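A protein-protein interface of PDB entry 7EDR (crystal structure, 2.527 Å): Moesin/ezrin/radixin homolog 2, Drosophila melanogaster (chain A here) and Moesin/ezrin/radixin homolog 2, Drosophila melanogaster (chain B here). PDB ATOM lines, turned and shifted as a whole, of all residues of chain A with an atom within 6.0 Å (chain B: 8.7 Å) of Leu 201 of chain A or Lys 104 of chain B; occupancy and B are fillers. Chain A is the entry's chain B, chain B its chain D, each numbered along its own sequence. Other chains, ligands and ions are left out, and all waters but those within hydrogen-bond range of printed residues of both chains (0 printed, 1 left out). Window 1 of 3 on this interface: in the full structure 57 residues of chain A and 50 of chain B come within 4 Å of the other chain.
The backbone NH (N) of Tyr 119 of chain A lies within hydrogen-bond range of the side-chain sulfur (SD) of Met 203 of chain A, at 3.4 Å. O of Gln 97 of chain B is in hydrogen-bond range of N of Glu 102 of chain B (3.1 Å). The side-chain amide oxygen of Asn 103 of chain B sits at hydrogen-bond distance from the backbone NH of Tyr 105 of chain B, 3.0 Å away.
Of the printed residues of chain B, Leu 201 of chain A touches Lys 104 (3.4 Å). Lys 104 of chain B touches four residues of chain A. Of the printed residues of chain A, Gln 97 of chain B touches Asp 202. Printed residues of chain B within 4 Å of Asp 200 of chain A: His 57, Lys 104 and Tyr 105. Leu 108 of chain B touches none of the printed residues of chain A. Ile 118 of chain A touches none of the printed residues of chain B. The nearest printed residue of chain B that does not touch Tyr 119 of chain A is Gln 97 of chain B (7.1 Å).
Among the printed residues, pairs that only touch across the chains: Leu 201 of chain A with Lys 104 of chain B (3.4 Å), Asp 200 of chain A with His 57 of chain B (3.4 Å), Asp 202 of chain A with Lys 104 of chain B (3.7 Å) and Asp 200 of chain A with Lys 104 of chain B (3.8 Å).
The side-chain hydroxyl of Tyr 119 of chain A lies close to the side-chain hydroxyl of Ser 94 of chain B (3.5 Å). The guanidinium group (NH1) of Arg 121 of chain A is in hydrogen-bond range of the side-chain hydroxyl (OG) of Ser 94 of chain B. O of Gln 199 of chain A is in hydrogen-bond range of NZ of Lys 104 of chain B (3.0 Å). O of Gln 199 of chain A lies within hydrogen-bond range of OH of Tyr 105 of chain B (3.3 Å). The side-chain carboxylate of Asp 200 of chain A lies close to the side-chain hydroxyl of Tyr 105 of chain B, at 3.1 Å. The side-chain amide nitrogen (NE2) of Gln 97 of chain B is in hydrogen-bond range of the side-chain carboxylate (OD2) of Asp 202 of chain A, 3.0 Å away.
Printed residues of chain A that touch a printed residue of chain B: Tyr 119, Arg 121, Gln 199, Asp 200, Leu 201 and Asp 202. Hydrophobic or aromatic side chains of chain A that line the printed part of chain B: Tyr 119. Of the 15 printed residues of chain B, 5 touch a printed residue of chain A. Hydrophobic or aromatic side chains of chain B that line the printed part of chain A: His 57 and Tyr 105. Among the printed residues, 10 pairs touch across the chains.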
ATOM      1  N   ILE A 113     -27.828 -13.008  -1.902  1.00  0.00           N
ATOM      2  CA  ILE A 113     -27.457 -11.633  -2.178  1.00  0.00           C
ATOM      3  C   ILE A 113     -28.357 -10.669  -1.406  1.00  0.00           C
ATOM      4  O   ILE A 113     -27.877  -9.790  -0.683  1.00  0.00           O
ATOM      5  CB  ILE A 113     -27.502 -11.395  -3.695  1.00  0.00           C
ATOM      6  CG1 ILE A 113     -26.390 -12.236  -4.358  1.00  0.00           C
ATOM      7  CG2 ILE A 113     -27.402  -9.919  -4.000  1.00  0.00           C
ATOM      8  CD1 ILE A 113     -26.341 -12.211  -5.867  1.00  0.00           C
ATOM      9  N   ILE A 118     -23.703 -13.169   0.828  1.00  0.00           N
ATOM     10  CA  ILE A 118     -22.547 -12.842   0.008  1.00  0.00           C
ATOM     11  C   ILE A 118     -22.604 -11.353  -0.332  1.00  0.00           C
ATOM     12  O   ILE A 118     -23.685 -10.783  -0.546  1.00  0.00           O
ATOM     13  CB  ILE A 118     -22.457 -13.724  -1.261  1.00  0.00           C
ATOM     14  CG1 ILE A 118     -23.521 -13.365  -2.281  1.00  0.00           C
ATOM     15  CG2 ILE A 118     -22.596 -15.216  -0.907  1.00  0.00           C
ATOM     16  CD1 ILE A 118     -23.527 -14.301  -3.463  1.00  0.00           C
ATOM     17  N   TYR A 119     -21.440 -10.712  -0.326  1.00  0.00           N
ATOM     18  CA  TYR A 119     -21.389  -9.289  -0.600  1.00  0.00           C
ATOM     19  C   TYR A 119     -21.654  -9.020  -2.074  1.00  0.00           C
ATOM     20  O   TYR A 119     -21.324  -9.824  -2.950  1.00  0.00           O
ATOM     21  CB  TYR A 119     -20.031  -8.724  -0.201  1.00  0.00           C
ATOM     22  CG  TYR A 119     -19.788  -7.312  -0.666  1.00  0.00           C
ATOM     23  CD1 TYR A 119     -20.248  -6.222   0.084  1.00  0.00           C
ATOM     24  CD2 TYR A 119     -19.091  -7.056  -1.850  1.00  0.00           C
ATOM     25  CE1 TYR A 119     -20.022  -4.924  -0.325  1.00  0.00           C
ATOM     26  CE2 TYR A 119     -18.866  -5.760  -2.268  1.00  0.00           C
ATOM     27  CZ  TYR A 119     -19.335  -4.694  -1.495  1.00  0.00           C
ATOM     28  OH  TYR A 119     -19.126  -3.391  -1.905  1.00  0.00           O
ATOM     29  N   CYS A 120     -22.235  -7.858  -2.343  1.00  0.00           N
ATOM     30  CA  CYS A 120     -22.515  -7.423  -3.700  1.00  0.00           C
ATOM     31  C   CYS A 120     -22.386  -5.901  -3.754  1.00  0.00           C
ATOM     32  O   CYS A 120     -22.797  -5.208  -2.820  1.00  0.00           O
ATOM     33  CB  CYS A 120     -23.909  -7.885  -4.130  1.00  0.00           C
ATOM     34  SG  CYS A 120     -24.339  -7.373  -5.786  1.00  0.00           S
ATOM     35  N   ARG A 121     -21.811  -5.386  -4.846  1.00  0.00           N
ATOM     36  CA  ARG A 121     -21.620  -3.950  -4.981  1.00  0.00           C
ATOM     37  C   ARG A 121     -22.948  -3.252  -5.270  1.00  0.00           C
ATOM     38  O   ARG A 121     -23.852  -3.849  -5.863  1.00  0.00           O
ATOM     39  CB  ARG A 121     -20.622  -3.634  -6.094  1.00  0.00           C
ATOM     40  CG  ARG A 121     -19.154  -3.834  -5.691  1.00  0.00           C
ATOM     41  CD  ARG A 121     -18.192  -2.999  -6.540  1.00  0.00           C
ATOM     42  NE  ARG A 121     -18.601  -1.592  -6.632  1.00  0.00           N
ATOM     43  CZ  ARG A 121     -18.424  -0.669  -5.681  1.00  0.00           C
ATOM     44  NH1 ARG A 121     -17.833  -0.978  -4.530  1.00  0.00           N
ATOM     45  NH2 ARG A 121     -18.856   0.572  -5.883  1.00  0.00           N
ATOM     46  N   ALA A 124     -24.034  -3.209  -9.020  1.00  0.00           N
ATOM     47  CA  ALA A 124     -24.384  -4.560  -9.461  1.00  0.00           C
ATOM     48  C   ALA A 124     -25.736  -4.997  -8.900  1.00  0.00           C
ATOM     49  O   ALA A 124     -26.514  -5.664  -9.596  1.00  0.00           O
ATOM     50  CB  ALA A 124     -23.292  -5.551  -9.056  1.00  0.00           C
ATOM     51  N   LEU A 128     -28.848  -6.687 -10.927  1.00  0.00           N
ATOM     52  CA  LEU A 128     -29.508  -7.904 -10.471  1.00  0.00           C
ATOM     53  C   LEU A 128     -30.980  -7.649 -10.195  1.00  0.00           C
ATOM     54  O   LEU A 128     -31.842  -8.482 -10.514  1.00  0.00           O
ATOM     55  CB  LEU A 128     -28.808  -8.441  -9.218  1.00  0.00           C
ATOM     56  CG  LEU A 128     -27.363  -8.880  -9.476  1.00  0.00           C
ATOM     57  CD1 LEU A 128     -26.703  -9.285  -8.191  1.00  0.00           C
ATOM     58  CD2 LEU A 128     -27.377 -10.024 -10.459  1.00  0.00           C
ATOM     59  N   ILE A 197     -23.885 -13.123 -13.613  1.00  0.00           N
ATOM     60  CA  ILE A 197     -23.313 -12.016 -12.864  1.00  0.00           C
ATOM     61  C   ILE A 197     -23.087 -12.382 -11.405  1.00  0.00           C
ATOM     62  O   ILE A 197     -22.064 -12.010 -10.824  1.00  0.00           O
ATOM     63  CB  ILE A 197     -24.218 -10.780 -13.026  1.00  0.00           C
ATOM     64  CG1 ILE A 197     -23.858 -10.110 -14.347  1.00  0.00           C
ATOM     65  CG2 ILE A 197     -24.048  -9.805 -11.853  1.00  0.00           C
ATOM     66  CD1 ILE A 197     -24.873  -9.294 -14.844  1.00  0.00           C
ATOM     67  N   ALA A 198     -24.012 -13.129 -10.795  1.00  0.00           N
ATOM     68  CA  ALA A 198     -23.798 -13.575  -9.422  1.00  0.00           C
ATOM     69  C   ALA A 198     -22.531 -14.408  -9.303  1.00  0.00           C
ATOM     70  O   ALA A 198     -21.796 -14.290  -8.317  1.00  0.00           O
ATOM     71  CB  ALA A 198     -24.992 -14.376  -8.918  1.00  0.00           C
ATOM     72  N   GLN A 199     -22.243 -15.247 -10.300  1.00  0.00           N
ATOM     73  CA  GLN A 199     -21.154 -16.190 -10.100  1.00  0.00           C
ATOM     74  C   GLN A 199     -19.786 -15.516 -10.122  1.00  0.00           C
ATOM     75  O   GLN A 199     -18.802 -16.132  -9.696  1.00  0.00           O
ATOM     76  CB  GLN A 199     -21.246 -17.326 -11.128  1.00  0.00           C
ATOM     77  CG  GLN A 199     -20.475 -17.140 -12.418  1.00  0.00           C
ATOM     78  CD  GLN A 199     -20.659 -18.322 -13.361  1.00  0.00           C
ATOM     79  OE1 GLN A 199     -20.873 -19.458 -12.931  1.00  0.00           O
ATOM     80  NE2 GLN A 199     -20.598 -18.056 -14.649  1.00  0.00           N
ATOM     81  N   ASP A 200     -19.709 -14.261 -10.553  1.00  0.00           N
ATOM     82  CA  ASP A 200     -18.454 -13.527 -10.550  1.00  0.00           C
ATOM     83  C   ASP A 200     -18.235 -12.741  -9.267  1.00  0.00           C
ATOM     84  O   ASP A 200     -17.183 -12.111  -9.115  1.00  0.00           O
ATOM     85  CB  ASP A 200     -18.378 -12.594 -11.774  1.00  0.00           C
ATOM     86  CG  ASP A 200     -18.072 -13.358 -13.080  1.00  0.00           C
ATOM     87  OD1 ASP A 200     -17.764 -14.572 -13.010  1.00  0.00           O
ATOM     88  OD2 ASP A 200     -18.120 -12.750 -14.170  1.00  0.00           O
ATOM     89  N   LEU A 201     -19.185 -12.763  -8.338  1.00  0.00           N
ATOM     90  CA  LEU A 201     -18.976 -12.109  -7.055  1.00  0.00           C
ATOM     91  C   LEU A 201     -17.903 -12.851  -6.263  1.00  0.00           C
ATOM     92  O   LEU A 201     -17.766 -14.075  -6.360  1.00  0.00           O
ATOM     93  CB  LEU A 201     -20.287 -12.051  -6.266  1.00  0.00           C
ATOM     94  CG  LEU A 201     -21.450 -11.315  -6.946  1.00  0.00           C
ATOM     95  CD1 LEU A 201     -22.675 -11.255  -6.034  1.00  0.00           C
ATOM     96  CD2 LEU A 201     -21.036  -9.912  -7.369  1.00  0.00           C
ATOM     97  N   ASP A 202     -17.125 -12.093  -5.481  1.00  0.00           N
ATOM     98  CA  ASP A 202     -15.990 -12.678  -4.761  1.00  0.00           C
ATOM     99  C   ASP A 202     -16.433 -13.786  -3.813  1.00  0.00           C
ATOM    100  O   ASP A 202     -15.720 -14.784  -3.630  1.00  0.00           O
ATOM    101  CB  ASP A 202     -15.241 -11.602  -3.963  1.00  0.00           C
ATOM    102  CG  ASP A 202     -14.614 -10.514  -4.848  1.00  0.00           C
ATOM    103  OD1 ASP A 202     -14.136 -10.838  -5.957  1.00  0.00           O
ATOM    104  OD2 ASP A 202     -14.594  -9.330  -4.424  1.00  0.00           O
ATOM    105  N   MET A 203     -17.585 -13.624  -3.174  1.00  0.00           N
ATOM    106  CA  MET A 203     -18.008 -14.561  -2.150  1.00  0.00           C
ATOM    107  C   MET A 203     -18.926 -15.652  -2.677  1.00  0.00           C
ATOM    108  O   MET A 203     -19.381 -16.486  -1.891  1.00  0.00           O
ATOM    109  CB  MET A 203     -18.699 -13.813  -0.999  1.00  0.00           C
ATOM    110  CG  MET A 203     -17.821 -12.730  -0.352  1.00  0.00           C
ATOM    111  SD  MET A 203     -18.604 -11.874   1.040  1.00  0.00           S
ATOM    112  CE  MET A 203     -18.846 -13.208   2.223  1.00  0.00           C
ATOM    113  N   TYR A 204     -19.214 -15.665  -3.974  1.00  0.00           N
ATOM    114  CA  TYR A 204     -20.123 -16.663  -4.525  1.00  0.00           C
ATOM    115  C   TYR A 204     -19.515 -18.055  -4.418  1.00  0.00           C
ATOM    116  O   TYR A 204     -18.338 -18.259  -4.731  1.00  0.00           O
ATOM    117  CB  TYR A 204     -20.441 -16.334  -5.975  1.00  0.00           C
ATOM    118  CG  TYR A 204     -21.221 -17.389  -6.710  1.00  0.00           C
ATOM    119  CD1 TYR A 204     -20.569 -18.380  -7.445  1.00  0.00           C
ATOM    120  CD2 TYR A 204     -22.614 -17.382  -6.703  1.00  0.00           C
ATOM    121  CE1 TYR A 204     -21.277 -19.348  -8.152  1.00  0.00           C
ATOM    122  CE2 TYR A 204     -23.334 -18.341  -7.402  1.00  0.00           C
ATOM    123  CZ  TYR A 204     -22.655 -19.316  -8.129  1.00  0.00           C
ATOM    124  OH  TYR A 204     -23.364 -20.264  -8.827  1.00  0.00           O
ATOM    125  N   VAL A 206     -18.504 -19.826  -1.889  1.00  0.00           N
ATOM    126  CA  VAL A 206     -17.442 -20.049  -0.917  1.00  0.00           C
ATOM    127  C   VAL A 206     -18.083 -20.445   0.400  1.00  0.00           C
ATOM    128  O   VAL A 206     -18.873 -19.685   0.969  1.00  0.00           O
ATOM    129  CB  VAL A 206     -16.562 -18.805  -0.725  1.00  0.00           C
ATOM    130  CG1 VAL A 206     -15.401 -19.137   0.189  1.00  0.00           C
ATOM    131  CG2 VAL A 206     -16.067 -18.279  -2.057  1.00  0.00           C
ATOM    132  N   HIS B  57     -14.532 -17.466 -20.252  1.00  0.00           N
ATOM    133  CA  HIS B  57     -14.787 -16.319 -19.396  1.00  0.00           C
ATOM    134  C   HIS B  57     -14.447 -15.006 -20.094  1.00  0.00           C
ATOM    135  O   HIS B  57     -15.209 -14.033 -19.990  1.00  0.00           O
ATOM    136  CB  HIS B  57     -14.003 -16.436 -18.102  1.00  0.00           C
ATOM    137  CG  HIS B  57     -14.234 -15.287 -17.183  1.00  0.00           C
ATOM    138  ND1 HIS B  57     -15.482 -14.987 -16.677  1.00  0.00           N
ATOM    139  CD2 HIS B  57     -13.397 -14.333 -16.716  1.00  0.00           C
ATOM    140  CE1 HIS B  57     -15.397 -13.919 -15.907  1.00  0.00           C
ATOM    141  NE2 HIS B  57     -14.144 -13.501 -15.918  1.00  0.00           N
ATOM    142  N   SER B  94     -13.888  -3.562  -1.280  1.00  0.00           N
ATOM    143  CA  SER B  94     -14.368  -3.688  -2.649  1.00  0.00           C
ATOM    144  C   SER B  94     -13.927  -2.506  -3.499  1.00  0.00           C
ATOM    145  O   SER B  94     -13.481  -2.686  -4.637  1.00  0.00           O
ATOM    146  CB  SER B  94     -15.892  -3.808  -2.667  1.00  0.00           C
ATOM    147  OG  SER B  94     -16.382  -3.679  -3.990  1.00  0.00           O
ATOM    148  N   GLN B  97     -10.282  -2.750  -4.263  1.00  0.00           N
ATOM    149  CA  GLN B  97     -10.082  -3.742  -5.308  1.00  0.00           C
ATOM    150  C   GLN B  97     -10.468  -3.189  -6.677  1.00  0.00           C
ATOM    151  O   GLN B  97      -9.805  -3.472  -7.681  1.00  0.00           O
ATOM    152  CB  GLN B  97     -10.887  -4.989  -4.952  1.00  0.00           C
ATOM    153  CG  GLN B  97     -11.052  -5.966  -6.063  1.00  0.00           C
ATOM    154  CD  GLN B  97     -12.214  -6.889  -5.791  1.00  0.00           C
ATOM    155  OE1 GLN B  97     -13.259  -6.796  -6.445  1.00  0.00           O
ATOM    156  NE2 GLN B  97     -12.053  -7.775  -4.798  1.00  0.00           N
ATOM    157  N   GLY B 101      -7.665  -2.421  -9.953  1.00  0.00           N
ATOM    158  CA  GLY B 101      -7.844  -3.181 -11.176  1.00  0.00           C
ATOM    159  C   GLY B 101      -7.926  -4.685 -11.003  1.00  0.00           C
ATOM    160  O   GLY B 101      -7.609  -5.428 -11.939  1.00  0.00           O
ATOM    161  N   GLU B 102      -8.356  -5.168  -9.843  1.00  0.00           N
ATOM    162  CA  GLU B 102      -8.333  -6.595  -9.548  1.00  0.00           C
ATOM    163  C   GLU B 102      -9.719  -7.219  -9.677  1.00  0.00           C
ATOM    164  O   GLU B 102     -10.731  -6.602  -9.317  1.00  0.00           O
ATOM    165  CB  GLU B 102      -7.804  -6.833  -8.139  1.00  0.00           C
ATOM    166  CG  GLU B 102      -6.427  -6.293  -7.899  1.00  0.00           C
ATOM    167  CD  GLU B 102      -6.150  -6.142  -6.423  1.00  0.00           C
ATOM    168  OE1 GLU B 102      -7.132  -6.083  -5.643  1.00  0.00           O
ATOM    169  OE2 GLU B 102      -4.959  -6.084  -6.046  1.00  0.00           O
ATOM    170  N   ASN B 103      -9.755  -8.461 -10.172  1.00  0.00           N
ATOM    171  CA  ASN B 103     -10.978  -9.257 -10.191  1.00  0.00           C
ATOM    172  C   ASN B 103     -10.699 -10.668  -9.695  1.00  0.00           C
ATOM    173  O   ASN B 103      -9.566 -11.158  -9.737  1.00  0.00           O
ATOM    174  CB  ASN B 103     -11.601  -9.343 -11.585  1.00  0.00           C
ATOM    175  CG  ASN B 103     -10.789 -10.180 -12.517  1.00  0.00           C
ATOM    176  OD1 ASN B 103     -11.057 -11.363 -12.707  1.00  0.00           O
ATOM    177  ND2 ASN B 103      -9.752  -9.577 -13.085  1.00  0.00           N
ATOM    178  N   LYS B 104     -11.781 -11.300  -9.236  1.00  0.00           N
ATOM    179  CA  LYS B 104     -11.778 -12.648  -8.681  1.00  0.00           C
ATOM    180  C   LYS B 104     -10.847 -13.601  -9.437  1.00  0.00           C
ATOM    181  O   LYS B 104      -9.970 -14.239  -8.838  1.00  0.00           O
ATOM    182  CB  LYS B 104     -13.225 -13.160  -8.696  1.00  0.00           C
ATOM    183  CG  LYS B 104     -13.576 -14.315  -7.766  1.00  0.00           C
ATOM    184  CD  LYS B 104     -14.888 -14.945  -8.233  1.00  0.00           C
ATOM    185  CE  LYS B 104     -15.320 -16.144  -7.393  1.00  0.00           C
ATOM    186  NZ  LYS B 104     -16.440 -16.873  -8.082  1.00  0.00           N
ATOM    187  N   TYR B 105     -10.993 -13.682 -10.765  1.00  0.00           N
ATOM    188  CA  TYR B 105     -10.287 -14.732 -11.494  1.00  0.00           C
ATOM    189  C   TYR B 105      -8.824 -14.385 -11.741  1.00  0.00           C
ATOM    190  O   TYR B 105      -7.959 -15.261 -11.640  1.00  0.00           O
ATOM    191  CB  TYR B 105     -11.028 -15.045 -12.795  1.00  0.00           C
ATOM    192  CG  TYR B 105     -12.428 -15.554 -12.506  1.00  0.00           C
ATOM    193  CD1 TYR B 105     -12.620 -16.703 -11.733  1.00  0.00           C
ATOM    194  CD2 TYR B 105     -13.558 -14.872 -12.964  1.00  0.00           C
ATOM    195  CE1 TYR B 105     -13.900 -17.172 -11.438  1.00  0.00           C
ATOM    196  CE2 TYR B 105     -14.843 -15.331 -12.679  1.00  0.00           C
ATOM    197  CZ  TYR B 105     -15.011 -16.481 -11.912  1.00  0.00           C
ATOM    198  OH  TYR B 105     -16.283 -16.949 -11.624  1.00  0.00           O
ATOM    199  N   SER B 106      -8.518 -13.119 -12.037  1.00  0.00           N
ATOM    200  CA  SER B 106      -7.120 -12.705 -12.164  1.00  0.00           C
ATOM    201  C   SER B 106      -6.342 -12.957 -10.879  1.00  0.00           C
ATOM    202  O   SER B 106      -5.184 -13.398 -10.915  1.00  0.00           O
ATOM    203  CB  SER B 106      -7.042 -11.225 -12.523  1.00  0.00           C
ATOM    204  OG  SER B 106      -7.490 -11.018 -13.845  1.00  0.00           O
ATOM    205  N   THR B 107      -6.953 -12.653  -9.734  1.00  0.00           N
ATOM    206  CA  THR B 107      -6.297 -12.887  -8.456  1.00  0.00           C
ATOM    207  C   THR B 107      -5.997 -14.368  -8.264  1.00  0.00           C
ATOM    208  O   THR B 107      -4.889 -14.746  -7.861  1.00  0.00           O
ATOM    209  CB  THR B 107      -7.185 -12.367  -7.328  1.00  0.00           C
ATOM    210  OG1 THR B 107      -7.414 -10.961  -7.507  1.00  0.00           O
ATOM    211  CG2 THR B 107      -6.543 -12.649  -5.968  1.00  0.00           C
ATOM    212  N   LEU B 108      -6.974 -15.226  -8.562  1.00  0.00           N
ATOM    213  CA  LEU B 108      -6.773 -16.654  -8.350  1.00  0.00           C
ATOM    214  C   LEU B 108      -5.689 -17.209  -9.266  1.00  0.00           C
ATOM    215  O   LEU B 108      -4.899 -18.061  -8.845  1.00  0.00           O
ATOM    216  CB  LEU B 108      -8.086 -17.403  -8.548  1.00  0.00           C
ATOM    217  CG  LEU B 108      -9.086 -17.279  -7.401  1.00  0.00           C
ATOM    218  CD1 LEU B 108     -10.487 -17.640  -7.873  1.00  0.00           C
ATOM    219  CD2 LEU B 108      -8.656 -18.156  -6.236  1.00  0.00           C
ATOM    220  N   LYS B 109      -5.631 -16.744 -10.519  1.00  0.00           N
ATOM    221  CA  LYS B 109      -4.616 -17.264 -11.423  1.00  0.00           C
ATOM    222  C   LYS B 109      -3.222 -16.875 -10.965  1.00  0.00           C
ATOM    223  O   LYS B 109      -2.307 -17.705 -10.996  1.00  0.00           O
ATOM    224  CB  LYS B 109      -4.853 -16.792 -12.851  1.00  0.00           C
ATOM    225  CG  LYS B 109      -4.056 -17.622 -13.855  1.00  0.00           C
ATOM    226  CD  LYS B 109      -4.410 -17.317 -15.303  1.00  0.00           C
ATOM    227  CE  LYS B 109      -3.850 -15.979 -15.742  1.00  0.00           C
ATOM    228  NZ  LYS B 109      -3.942 -15.816 -17.218  1.00  0.00           N
ATOM    229  N   LYS B 110      -3.043 -15.633 -10.503  1.00  0.00           N
ATOM    230  CA  LYS B 110      -1.721 -15.224 -10.030  1.00  0.00           C
ATOM    231  C   LYS B 110      -1.321 -15.989  -8.770  1.00  0.00           C
ATOM    232  O   LYS B 110      -0.183 -16.456  -8.661  1.00  0.00           O
ATOM    233  CB  LYS B 110      -1.680 -13.714  -9.784  1.00  0.00           C
ATOM    234  CG  LYS B 110      -0.262 -13.156  -9.618  1.00  0.00           C
ATOM    235  CD  LYS B 110      -0.205 -12.011  -8.603  1.00  0.00           C
ATOM    236  CE  LYS B 110      -0.689 -12.462  -7.218  1.00  0.00           C
ATOM    237  NZ  LYS B 110      -0.522 -11.414  -6.151  1.00  0.00           N
ATOM    238  N   LEU B 111      -2.241 -16.131  -7.814  1.00  0.00           N
ATOM    239  CA  LEU B 111      -1.958 -16.922  -6.618  1.00  0.00           C
ATOM    240  C   LEU B 111      -1.512 -18.339  -6.967  1.00  0.00           C
ATOM    241  O   LEU B 111      -0.552 -18.863  -6.383  1.00  0.00           O
ATOM    242  CB  LEU B 111      -3.198 -16.974  -5.726  1.00  0.00           C
ATOM    243  CG  LEU B 111      -3.606 -15.694  -5.003  1.00  0.00           C
ATOM    244  CD1 LEU B 111      -4.899 -15.910  -4.258  1.00  0.00           C
ATOM    245  CD2 LEU B 111      -2.493 -15.273  -4.058  1.00  0.00           C
ATOM    246  N   LYS B 112      -2.206 -18.983  -7.904  1.00  0.00           N
ATOM    247  CA  LYS B 112      -1.856 -20.346  -8.274  1.00  0.00           C
ATOM    248  C   LYS B 112      -0.604 -20.413  -9.130  1.00  0.00           C
ATOM    249  O   LYS B 112      -0.008 -21.488  -9.242  1.00  0.00           O
ATOM    250  CB  LYS B 112      -3.019 -21.008  -9.012  1.00  0.00           C
ATOM    251  CG  LYS B 112      -4.085 -21.547  -8.079  1.00  0.00           C
ATOM    252  CD  LYS B 112      -5.385 -21.806  -8.822  1.00  0.00           C
ATOM    253  CE  LYS B 112      -6.523 -21.996  -7.839  1.00  0.00           C
ATOM    254  NZ  LYS B 112      -7.801 -22.194  -8.549  1.00  0.00           N
